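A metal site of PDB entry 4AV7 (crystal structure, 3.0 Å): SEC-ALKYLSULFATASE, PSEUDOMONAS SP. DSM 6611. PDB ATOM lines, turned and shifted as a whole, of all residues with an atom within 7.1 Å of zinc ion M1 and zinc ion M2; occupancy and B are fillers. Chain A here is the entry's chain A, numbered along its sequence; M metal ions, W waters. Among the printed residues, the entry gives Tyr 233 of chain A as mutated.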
ATOM      1  N   PRO A 132     -12.743  28.622 -27.636  1.00  0.00           N
ATOM      2  CA  PRO A 132     -13.067  29.199 -26.321  1.00  0.00           C
ATOM      3  C   PRO A 132     -13.491  28.145 -25.292  1.00  0.00           C
ATOM      4  O   PRO A 132     -13.156  28.292 -24.123  1.00  0.00           O
ATOM      5  CB  PRO A 132     -14.235  30.133 -26.609  1.00  0.00           C
ATOM      6  CG  PRO A 132     -14.608  29.920 -28.055  1.00  0.00           C
ATOM      7  CD  PRO A 132     -13.399  29.347 -28.728  1.00  0.00           C
ATOM      8  N   ALA A 133     -14.193  27.099 -25.727  1.00  0.00           N
ATOM      9  CA  ALA A 133     -14.673  26.015 -24.853  1.00  0.00           C
ATOM     10  C   ALA A 133     -13.775  24.761 -24.828  1.00  0.00           C
ATOM     11  O   ALA A 133     -12.721  24.722 -25.452  1.00  0.00           O
ATOM     12  CB  ALA A 133     -16.088  25.639 -25.251  1.00  0.00           C
ATOM     13  N   ASN A 134     -14.207  23.734 -24.114  1.00  0.00           N
ATOM     14  CA  ASN A 134     -13.506  22.454 -24.136  1.00  0.00           C
ATOM     15  C   ASN A 134     -14.308  21.304 -24.801  1.00  0.00           C
ATOM     16  O   ASN A 134     -15.545  21.382 -25.011  1.00  0.00           O
ATOM     17  CB  ASN A 134     -13.083  22.075 -22.716  1.00  0.00           C
ATOM     18  CG  ASN A 134     -12.098  23.059 -22.085  1.00  0.00           C
ATOM     19  OD1 ASN A 134     -11.504  23.922 -22.772  1.00  0.00           O
ATOM     20  ND2 ASN A 134     -11.906  22.937 -20.761  1.00  0.00           N
ATOM     21  N   ASP A 148     -19.951  18.015 -25.683  1.00  0.00           N
ATOM     22  CA  ASP A 148     -19.773  19.293 -26.395  1.00  0.00           C
ATOM     23  C   ASP A 148     -18.833  19.190 -27.581  1.00  0.00           C
ATOM     24  O   ASP A 148     -17.862  18.440 -27.554  1.00  0.00           O
ATOM     25  CB  ASP A 148     -19.365  20.419 -25.461  1.00  0.00           C
ATOM     26  CG  ASP A 148     -20.408  20.691 -24.406  1.00  0.00           C
ATOM     27  OD1 ASP A 148     -21.605  20.420 -24.682  1.00  0.00           O
ATOM     28  OD2 ASP A 148     -20.046  21.167 -23.306  1.00  0.00           O
ATOM     29  N   SER A 178     -24.126  19.875 -23.435  1.00  0.00           N
ATOM     30  CA  SER A 178     -24.303  20.184 -22.033  1.00  0.00           C
ATOM     31  C   SER A 178     -25.226  21.408 -21.790  1.00  0.00           C
ATOM     32  O   SER A 178     -25.853  21.517 -20.723  1.00  0.00           O
ATOM     33  CB  SER A 178     -22.946  20.427 -21.410  1.00  0.00           C
ATOM     34  OG  SER A 178     -22.362  21.558 -22.026  1.00  0.00           O
ATOM     35  N   HIS A 179     -25.321  22.295 -22.790  1.00  0.00           N
ATOM     36  CA  HIS A 179     -26.243  23.435 -22.737  1.00  0.00           C
ATOM     37  C   HIS A 179     -26.434  24.136 -24.069  1.00  0.00           C
ATOM     38  O   HIS A 179     -25.745  23.824 -25.027  1.00  0.00           O
ATOM     39  CB  HIS A 179     -25.846  24.446 -21.657  1.00  0.00           C
ATOM     40  CG  HIS A 179     -24.443  25.014 -21.793  1.00  0.00           C
ATOM     41  ND1 HIS A 179     -23.349  24.346 -21.440  1.00  0.00           N
ATOM     42  CD2 HIS A 179     -24.011  26.272 -22.216  1.00  0.00           C
ATOM     43  CE1 HIS A 179     -22.266  25.121 -21.633  1.00  0.00           C
ATOM     44  NE2 HIS A 179     -22.682  26.298 -22.108  1.00  0.00           N
ATOM     45  N   SER A 180     -27.347  25.104 -24.132  1.00  0.00           N
ATOM     46  CA  SER A 180     -27.696  25.717 -25.414  1.00  0.00           C
ATOM     47  C   SER A 180     -26.820  26.919 -25.728  1.00  0.00           C
ATOM     48  O   SER A 180     -27.334  27.971 -26.129  1.00  0.00           O
ATOM     49  CB  SER A 180     -29.171  26.111 -25.465  1.00  0.00           C
ATOM     50  OG  SER A 180     -29.493  26.970 -24.385  1.00  0.00           O
ATOM     51  N   HIS A 181     -25.507  26.761 -25.562  1.00  0.00           N
ATOM     52  CA  HIS A 181     -24.545  27.793 -25.964  1.00  0.00           C
ATOM     53  C   HIS A 181     -23.695  27.406 -27.146  1.00  0.00           C
ATOM     54  O   HIS A 181     -23.074  26.329 -27.168  1.00  0.00           O
ATOM     55  CB  HIS A 181     -23.637  28.236 -24.808  1.00  0.00           C
ATOM     56  CG  HIS A 181     -24.306  29.142 -23.784  1.00  0.00           C
ATOM     57  ND1 HIS A 181     -23.792  29.333 -22.534  1.00  0.00           N
ATOM     58  CD2 HIS A 181     -25.472  29.902 -23.847  1.00  0.00           C
ATOM     59  CE1 HIS A 181     -24.583  30.164 -21.841  1.00  0.00           C
ATOM     60  NE2 HIS A 181     -25.624  30.516 -22.643  1.00  0.00           N
ATOM     61  N   ILE A 182     -23.647  28.298 -28.141  1.00  0.00           N
ATOM     62  CA  ILE A 182     -22.952  28.086 -29.416  1.00  0.00           C
ATOM     63  C   ILE A 182     -21.523  27.510 -29.295  1.00  0.00           C
ATOM     64  O   ILE A 182     -21.073  26.753 -30.155  1.00  0.00           O
ATOM     65  CB  ILE A 182     -22.981  29.382 -30.238  1.00  0.00           C
ATOM     66  CG1 ILE A 182     -22.945  29.057 -31.739  1.00  0.00           C
ATOM     67  CG2 ILE A 182     -21.839  30.311 -29.806  1.00  0.00           C
ATOM     68  CD1 ILE A 182     -23.255  30.237 -32.619  1.00  0.00           C
ATOM     69  N   ASP A 183     -20.817  27.836 -28.223  1.00  0.00           N
ATOM     70  CA  ASP A 183     -19.472  27.316 -28.011  1.00  0.00           C
ATOM     71  C   ASP A 183     -19.477  25.840 -27.608  1.00  0.00           C
ATOM     72  O   ASP A 183     -18.427  25.287 -27.239  1.00  0.00           O
ATOM     73  CB  ASP A 183     -18.687  28.184 -26.984  1.00  0.00           C
ATOM     74  CG  ASP A 183     -19.434  28.415 -25.653  1.00  0.00           C
ATOM     75  OD1 ASP A 183     -20.660  28.673 -25.697  1.00  0.00           O
ATOM     76  OD2 ASP A 183     -18.808  28.378 -24.556  1.00  0.00           O
ATOM     77  N   HIS A 184     -20.650  25.198 -27.654  1.00  0.00           N
ATOM     78  CA  HIS A 184     -20.758  23.807 -27.244  1.00  0.00           C
ATOM     79  C   HIS A 184     -21.480  22.947 -28.241  1.00  0.00           C
ATOM     80  O   HIS A 184     -21.255  21.715 -28.261  1.00  0.00           O
ATOM     81  CB  HIS A 184     -21.386  23.717 -25.869  1.00  0.00           C
ATOM     82  CG  HIS A 184     -20.669  24.525 -24.826  1.00  0.00           C
ATOM     83  ND1 HIS A 184     -19.767  23.988 -23.991  1.00  0.00           N
ATOM     84  CD2 HIS A 184     -20.745  25.872 -24.495  1.00  0.00           C
ATOM     85  CE1 HIS A 184     -19.288  24.943 -23.184  1.00  0.00           C
ATOM     86  NE2 HIS A 184     -19.893  26.093 -23.492  1.00  0.00           N
ATOM     87  N   TYR A 233     -15.585  39.380 -26.842  1.00  0.00           N
ATOM     88  CA  TYR A 233     -14.347  38.599 -27.061  1.00  0.00           C
ATOM     89  C   TYR A 233     -13.229  39.401 -27.753  1.00  0.00           C
ATOM     90  O   TYR A 233     -12.170  38.835 -28.071  1.00  0.00           O
ATOM     91  CB  TYR A 233     -14.653  37.346 -27.874  1.00  0.00           C
ATOM     92  CG  TYR A 233     -15.659  36.441 -27.227  1.00  0.00           C
ATOM     93  CD1 TYR A 233     -15.268  35.505 -26.274  1.00  0.00           C
ATOM     94  CD2 TYR A 233     -17.016  36.514 -27.580  1.00  0.00           C
ATOM     95  CE1 TYR A 233     -16.184  34.658 -25.689  1.00  0.00           C
ATOM     96  CE2 TYR A 233     -17.951  35.671 -26.980  1.00  0.00           C
ATOM     97  CZ  TYR A 233     -17.517  34.735 -26.046  1.00  0.00           C
ATOM     98  OH  TYR A 233     -18.393  33.877 -25.428  1.00  0.00           O
ATOM     99  N   LEU A 249     -12.691  32.720 -19.635  1.00  0.00           N
ATOM    100  CA  LEU A 249     -12.892  31.294 -19.696  1.00  0.00           C
ATOM    101  C   LEU A 249     -12.328  30.763 -20.988  1.00  0.00           C
ATOM    102  O   LEU A 249     -12.672  29.655 -21.434  1.00  0.00           O
ATOM    103  CB  LEU A 249     -14.364  30.953 -19.590  1.00  0.00           C
ATOM    104  CG  LEU A 249     -15.137  31.530 -18.407  1.00  0.00           C
ATOM    105  CD1 LEU A 249     -16.566  31.023 -18.464  1.00  0.00           C
ATOM    106  CD2 LEU A 249     -14.488  31.193 -17.073  1.00  0.00           C
ATOM    107  N   GLU A 291     -26.811  28.764 -15.819  1.00  0.00           N
ATOM    108  CA  GLU A 291     -25.871  29.395 -16.769  1.00  0.00           C
ATOM    109  C   GLU A 291     -26.489  29.581 -18.153  1.00  0.00           C
ATOM    110  O   GLU A 291     -26.163  30.536 -18.861  1.00  0.00           O
ATOM    111  CB  GLU A 291     -24.581  28.603 -16.886  1.00  0.00           C
ATOM    112  CG  GLU A 291     -23.498  29.292 -17.732  1.00  0.00           C
ATOM    113  CD  GLU A 291     -23.266  28.676 -19.126  1.00  0.00           C
ATOM    114  OE1 GLU A 291     -23.788  27.573 -19.459  1.00  0.00           O
ATOM    115  OE2 GLU A 291     -22.504  29.289 -19.911  1.00  0.00           O
ATOM    116  N   ALA A 292     -27.381  28.662 -18.505  1.00  0.00           N
ATOM    117  CA  ALA A 292     -28.056  28.643 -19.788  1.00  0.00           C
ATOM    118  C   ALA A 292     -29.505  28.241 -19.506  1.00  0.00           C
ATOM    119  O   ALA A 292     -29.749  27.508 -18.539  1.00  0.00           O
ATOM    120  CB  ALA A 292     -27.420  27.621 -20.692  1.00  0.00           C
ATOM    121  N   ASP A 295     -29.737  23.524 -19.954  1.00  0.00           N
ATOM    122  CA  ASP A 295     -28.417  23.277 -19.340  1.00  0.00           C
ATOM    123  C   ASP A 295     -28.483  22.083 -18.370  1.00  0.00           C
ATOM    124  O   ASP A 295     -29.519  21.866 -17.718  1.00  0.00           O
ATOM    125  CB  ASP A 295     -27.965  24.576 -18.634  1.00  0.00           C
ATOM    126  CG  ASP A 295     -26.650  24.443 -17.876  1.00  0.00           C
ATOM    127  OD1 ASP A 295     -25.652  23.929 -18.429  1.00  0.00           O
ATOM    128  OD2 ASP A 295     -26.607  24.907 -16.714  1.00  0.00           O
ATOM    129  N   ALA A 309     -20.072  21.252 -16.640  1.00  0.00           N
ATOM    130  CA  ALA A 309     -20.224  22.054 -17.848  1.00  0.00           C
ATOM    131  C   ALA A 309     -19.747  23.522 -17.677  1.00  0.00           C
ATOM    132  O   ALA A 309     -18.543  23.765 -17.550  1.00  0.00           O
ATOM    133  CB  ALA A 309     -21.653  21.995 -18.343  1.00  0.00           C
ATOM    134  N   ASP A 310     -20.660  24.472 -17.664  1.00  0.00           N
ATOM    135  CA  ASP A 310     -20.321  25.883 -17.447  1.00  0.00           C
ATOM    136  C   ASP A 310     -20.889  26.425 -16.124  1.00  0.00           C
ATOM    137  O   ASP A 310     -20.778  27.608 -15.841  1.00  0.00           O
ATOM    138  CB  ASP A 310     -20.798  26.766 -18.625  1.00  0.00           C
ATOM    139  CG  ASP A 310     -19.983  26.563 -19.897  1.00  0.00           C
ATOM    140  OD1 ASP A 310     -19.209  25.568 -19.980  1.00  0.00           O
ATOM    141  OD2 ASP A 310     -20.129  27.404 -20.824  1.00  0.00           O
ATOM    142  N   ASN A 311     -21.439  25.555 -15.299  1.00  0.00           N
ATOM    143  CA  ASN A 311     -22.023  25.977 -14.051  1.00  0.00           C
ATOM    144  C   ASN A 311     -21.069  26.357 -12.928  1.00  0.00           C
ATOM    145  O   ASN A 311     -21.468  27.055 -11.996  1.00  0.00           O
ATOM    146  CB  ASN A 311     -23.013  24.924 -13.586  1.00  0.00           C
ATOM    147  CG  ASN A 311     -24.050  24.616 -14.647  1.00  0.00           C
ATOM    148  OD1 ASN A 311     -24.286  25.436 -15.546  1.00  0.00           O
ATOM    149  ND2 ASN A 311     -24.650  23.441 -14.568  1.00  0.00           N
ATOM    150  N   HIS A 317     -18.983  33.781 -13.185  1.00  0.00           N
ATOM    151  CA  HIS A 317     -19.636  33.738 -14.508  1.00  0.00           C
ATOM    152  C   HIS A 317     -20.618  34.898 -14.614  1.00  0.00           C
ATOM    153  O   HIS A 317     -20.882  35.562 -13.630  1.00  0.00           O
ATOM    154  CB  HIS A 317     -20.298  32.397 -14.744  1.00  0.00           C
ATOM    155  CG  HIS A 317     -20.438  31.982 -16.204  1.00  0.00           C
ATOM    156  ND1 HIS A 317     -20.712  32.843 -17.196  1.00  0.00           N
ATOM    157  CD2 HIS A 317     -20.397  30.718 -16.785  1.00  0.00           C
ATOM    158  CE1 HIS A 317     -20.813  32.177 -18.351  1.00  0.00           C
ATOM    159  NE2 HIS A 317     -20.621  30.871 -18.097  1.00  0.00           N
ATOM    160  N   ARG A 323     -22.688  39.896 -24.738  1.00  0.00           N
ATOM    161  CA  ARG A 323     -23.183  39.705 -26.097  1.00  0.00           C
ATOM    162  C   ARG A 323     -24.695  39.843 -26.123  1.00  0.00           C
ATOM    163  O   ARG A 323     -25.267  40.165 -27.172  1.00  0.00           O
ATOM    164  CB  ARG A 323     -22.765  38.336 -26.622  1.00  0.00           C
ATOM    165  CG  ARG A 323     -23.469  37.164 -25.934  1.00  0.00           C
ATOM    166  CD  ARG A 323     -22.773  35.867 -26.243  1.00  0.00           C
ATOM    167  NE  ARG A 323     -23.109  34.842 -25.264  1.00  0.00           N
ATOM    168  CZ  ARG A 323     -24.120  34.004 -25.389  1.00  0.00           C
ATOM    169  NH1 ARG A 323     -24.910  34.059 -26.451  1.00  0.00           N
ATOM    170  NH2 ARG A 323     -24.337  33.083 -24.453  1.00  0.00           N
ATOM    171  N   ARG A 328     -29.988  35.351 -16.018  1.00  0.00           N
ATOM    172  CA  ARG A 328     -29.790  34.093 -15.372  1.00  0.00           C
ATOM    173  C   ARG A 328     -30.188  34.110 -13.901  1.00  0.00           C
ATOM    174  O   ARG A 328     -30.079  35.126 -13.222  1.00  0.00           O
ATOM    175  CB  ARG A 328     -28.343  33.705 -15.568  1.00  0.00           C
ATOM    176  CG  ARG A 328     -28.106  33.444 -17.039  1.00  0.00           C
ATOM    177  CD  ARG A 328     -26.649  33.406 -17.365  1.00  0.00           C
ATOM    178  NE  ARG A 328     -26.498  33.216 -18.790  1.00  0.00           N
ATOM    179  CZ  ARG A 328     -25.367  33.469 -19.464  1.00  0.00           C
ATOM    180  NH1 ARG A 328     -24.294  33.951 -18.847  1.00  0.00           N
ATOM    181  NH2 ARG A 328     -25.316  33.245 -20.767  1.00  0.00           N
ATOM    182  N   GLN A 354     -16.346  22.432 -18.925  1.00  0.00           N
ATOM    183  CA  GLN A 354     -16.323  22.675 -20.355  1.00  0.00           C
ATOM    184  C   GLN A 354     -15.566  23.972 -20.770  1.00  0.00           C
ATOM    185  O   GLN A 354     -15.564  24.394 -21.947  1.00  0.00           O
ATOM    186  CB  GLN A 354     -17.732  22.578 -20.908  1.00  0.00           C
ATOM    187  CG  GLN A 354     -18.269  21.138 -20.915  1.00  0.00           C
ATOM    188  CD  GLN A 354     -17.314  20.113 -21.552  1.00  0.00           C
ATOM    189  OE1 GLN A 354     -16.787  19.243 -20.851  1.00  0.00           O
ATOM    190  NE2 GLN A 354     -17.111  20.198 -22.876  1.00  0.00           N
ATOM    191  N   HIS A 355     -14.923  24.599 -19.781  1.00  0.00           N
ATOM    192  CA  HIS A 355     -14.070  25.770 -19.945  1.00  0.00           C
ATOM    193  C   HIS A 355     -13.053  25.596 -18.860  1.00  0.00           C
ATOM    194  O   HIS A 355     -13.366  25.028 -17.789  1.00  0.00           O
ATOM    195  CB  HIS A 355     -14.802  27.086 -19.705  1.00  0.00           C
ATOM    196  CG  HIS A 355     -15.699  27.536 -20.830  1.00  0.00           C
ATOM    197  ND1 HIS A 355     -15.238  28.218 -21.889  1.00  0.00           N
ATOM    198  CD2 HIS A 355     -17.089  27.426 -20.999  1.00  0.00           C
ATOM    199  CE1 HIS A 355     -16.270  28.508 -22.718  1.00  0.00           C
ATOM    200  NE2 HIS A 355     -17.403  28.017 -22.164  1.00  0.00           N
ATOM    201  N   TYR A 417     -14.462  36.726 -15.824  1.00  0.00           N
ATOM    202  CA  TYR A 417     -15.525  36.575 -16.825  1.00  0.00           C
ATOM    203  C   TYR A 417     -16.744  37.453 -16.461  1.00  0.00           C
ATOM    204  O   TYR A 417     -16.958  38.540 -17.031  1.00  0.00           O
ATOM    205  CB  TYR A 417     -15.925  35.095 -16.969  1.00  0.00           C
ATOM    206  CG  TYR A 417     -16.477  34.768 -18.337  1.00  0.00           C
ATOM    207  CD1 TYR A 417     -15.643  34.777 -19.468  1.00  0.00           C
ATOM    208  CD2 TYR A 417     -17.826  34.457 -18.517  1.00  0.00           C
ATOM    209  CE1 TYR A 417     -16.130  34.483 -20.725  1.00  0.00           C
ATOM    210  CE2 TYR A 417     -18.326  34.168 -19.771  1.00  0.00           C
ATOM    211  CZ  TYR A 417     -17.472  34.178 -20.876  1.00  0.00           C
ATOM    212  OH  TYR A 417     -17.948  33.893 -22.134  1.00  0.00           O
HETATM  213 ZN    ZN M   1     -19.318  27.754 -22.666  1.00  0.00          ZN
HETATM  214 ZN    ZN M   2     -22.126  28.361 -21.553  1.00  0.00          ZN
HETATM  215  O   HOH W   1     -20.767  30.068 -23.391  1.00  0.00           O
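A ring nitrogen (NE2) of His 317 lies close to the side-chain carboxylate of Glu 291 (3.1 Å). NE of Arg 328 sits at hydrogen-bond distance from O of Glu 291. ND1 of His 184 is in hydrogen-bond range of OD2 of Asp 148 (2.9 Å). ND1 of His 355 lies within hydrogen-bond range of O of Leu 249, 3.0 Å away. ND1 of His 355 sits at hydrogen-bond distance from O of Pro 132, at 3.1 Å. NE2 of His 181 sits at hydrogen-bond distance from NH2 of Arg 328, 3.3 Å away. A ring nitrogen (NE2) of His 181 lies within hydrogen-bond range of the guanidinium group (NH2) of Arg 323, at 3.4 Å. A ring nitrogen (ND1) of His 179 is in hydrogen-bond range of the side-chain hydroxyl (OG) of Ser 178 (3.0 Å).
Within 4 Å of zinc ion M1: His 179, Asp 183, His 184, Asp 310 and His 355. The nearest printed residue that does not touch zinc ion M1 is Glu 291 (4.5 Å).
Five residues have an atom within 4 Å of zinc ion M2: His 179, His 181, His 184, Glu 291 and Asp 310. The nearest printed residue that does not touch zinc ion M2 is Asp 183 (4.4 Å).
Zinc ion M1 is bound by a ring nitrogen (NE2) of His 184. Zinc ion M1 is bound by a ring nitrogen (NE2) of His 355, at 2.0 Å. OD2 of Asp 310 binds zinc ion M1 (2.0 Å). OD2 of Asp 183 binds zinc ion M1 (2.1 Å). Zinc ion M1 has four donor atoms within binding distance. Slightly farther from zinc ion M1 lies water W1 (2.8 Å).
Zinc ion M2 is bound by OE2 of Glu 291 (1.9 Å), ND1 of His 181 (2.2 Å), NE2 of His 179 (2.2 Å) and OD2 of Asp 310 (2.3 Å). Slightly farther from zinc ion M2 lies the side-chain carboxylate (OE1) of Glu 291 (2.8 Å).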
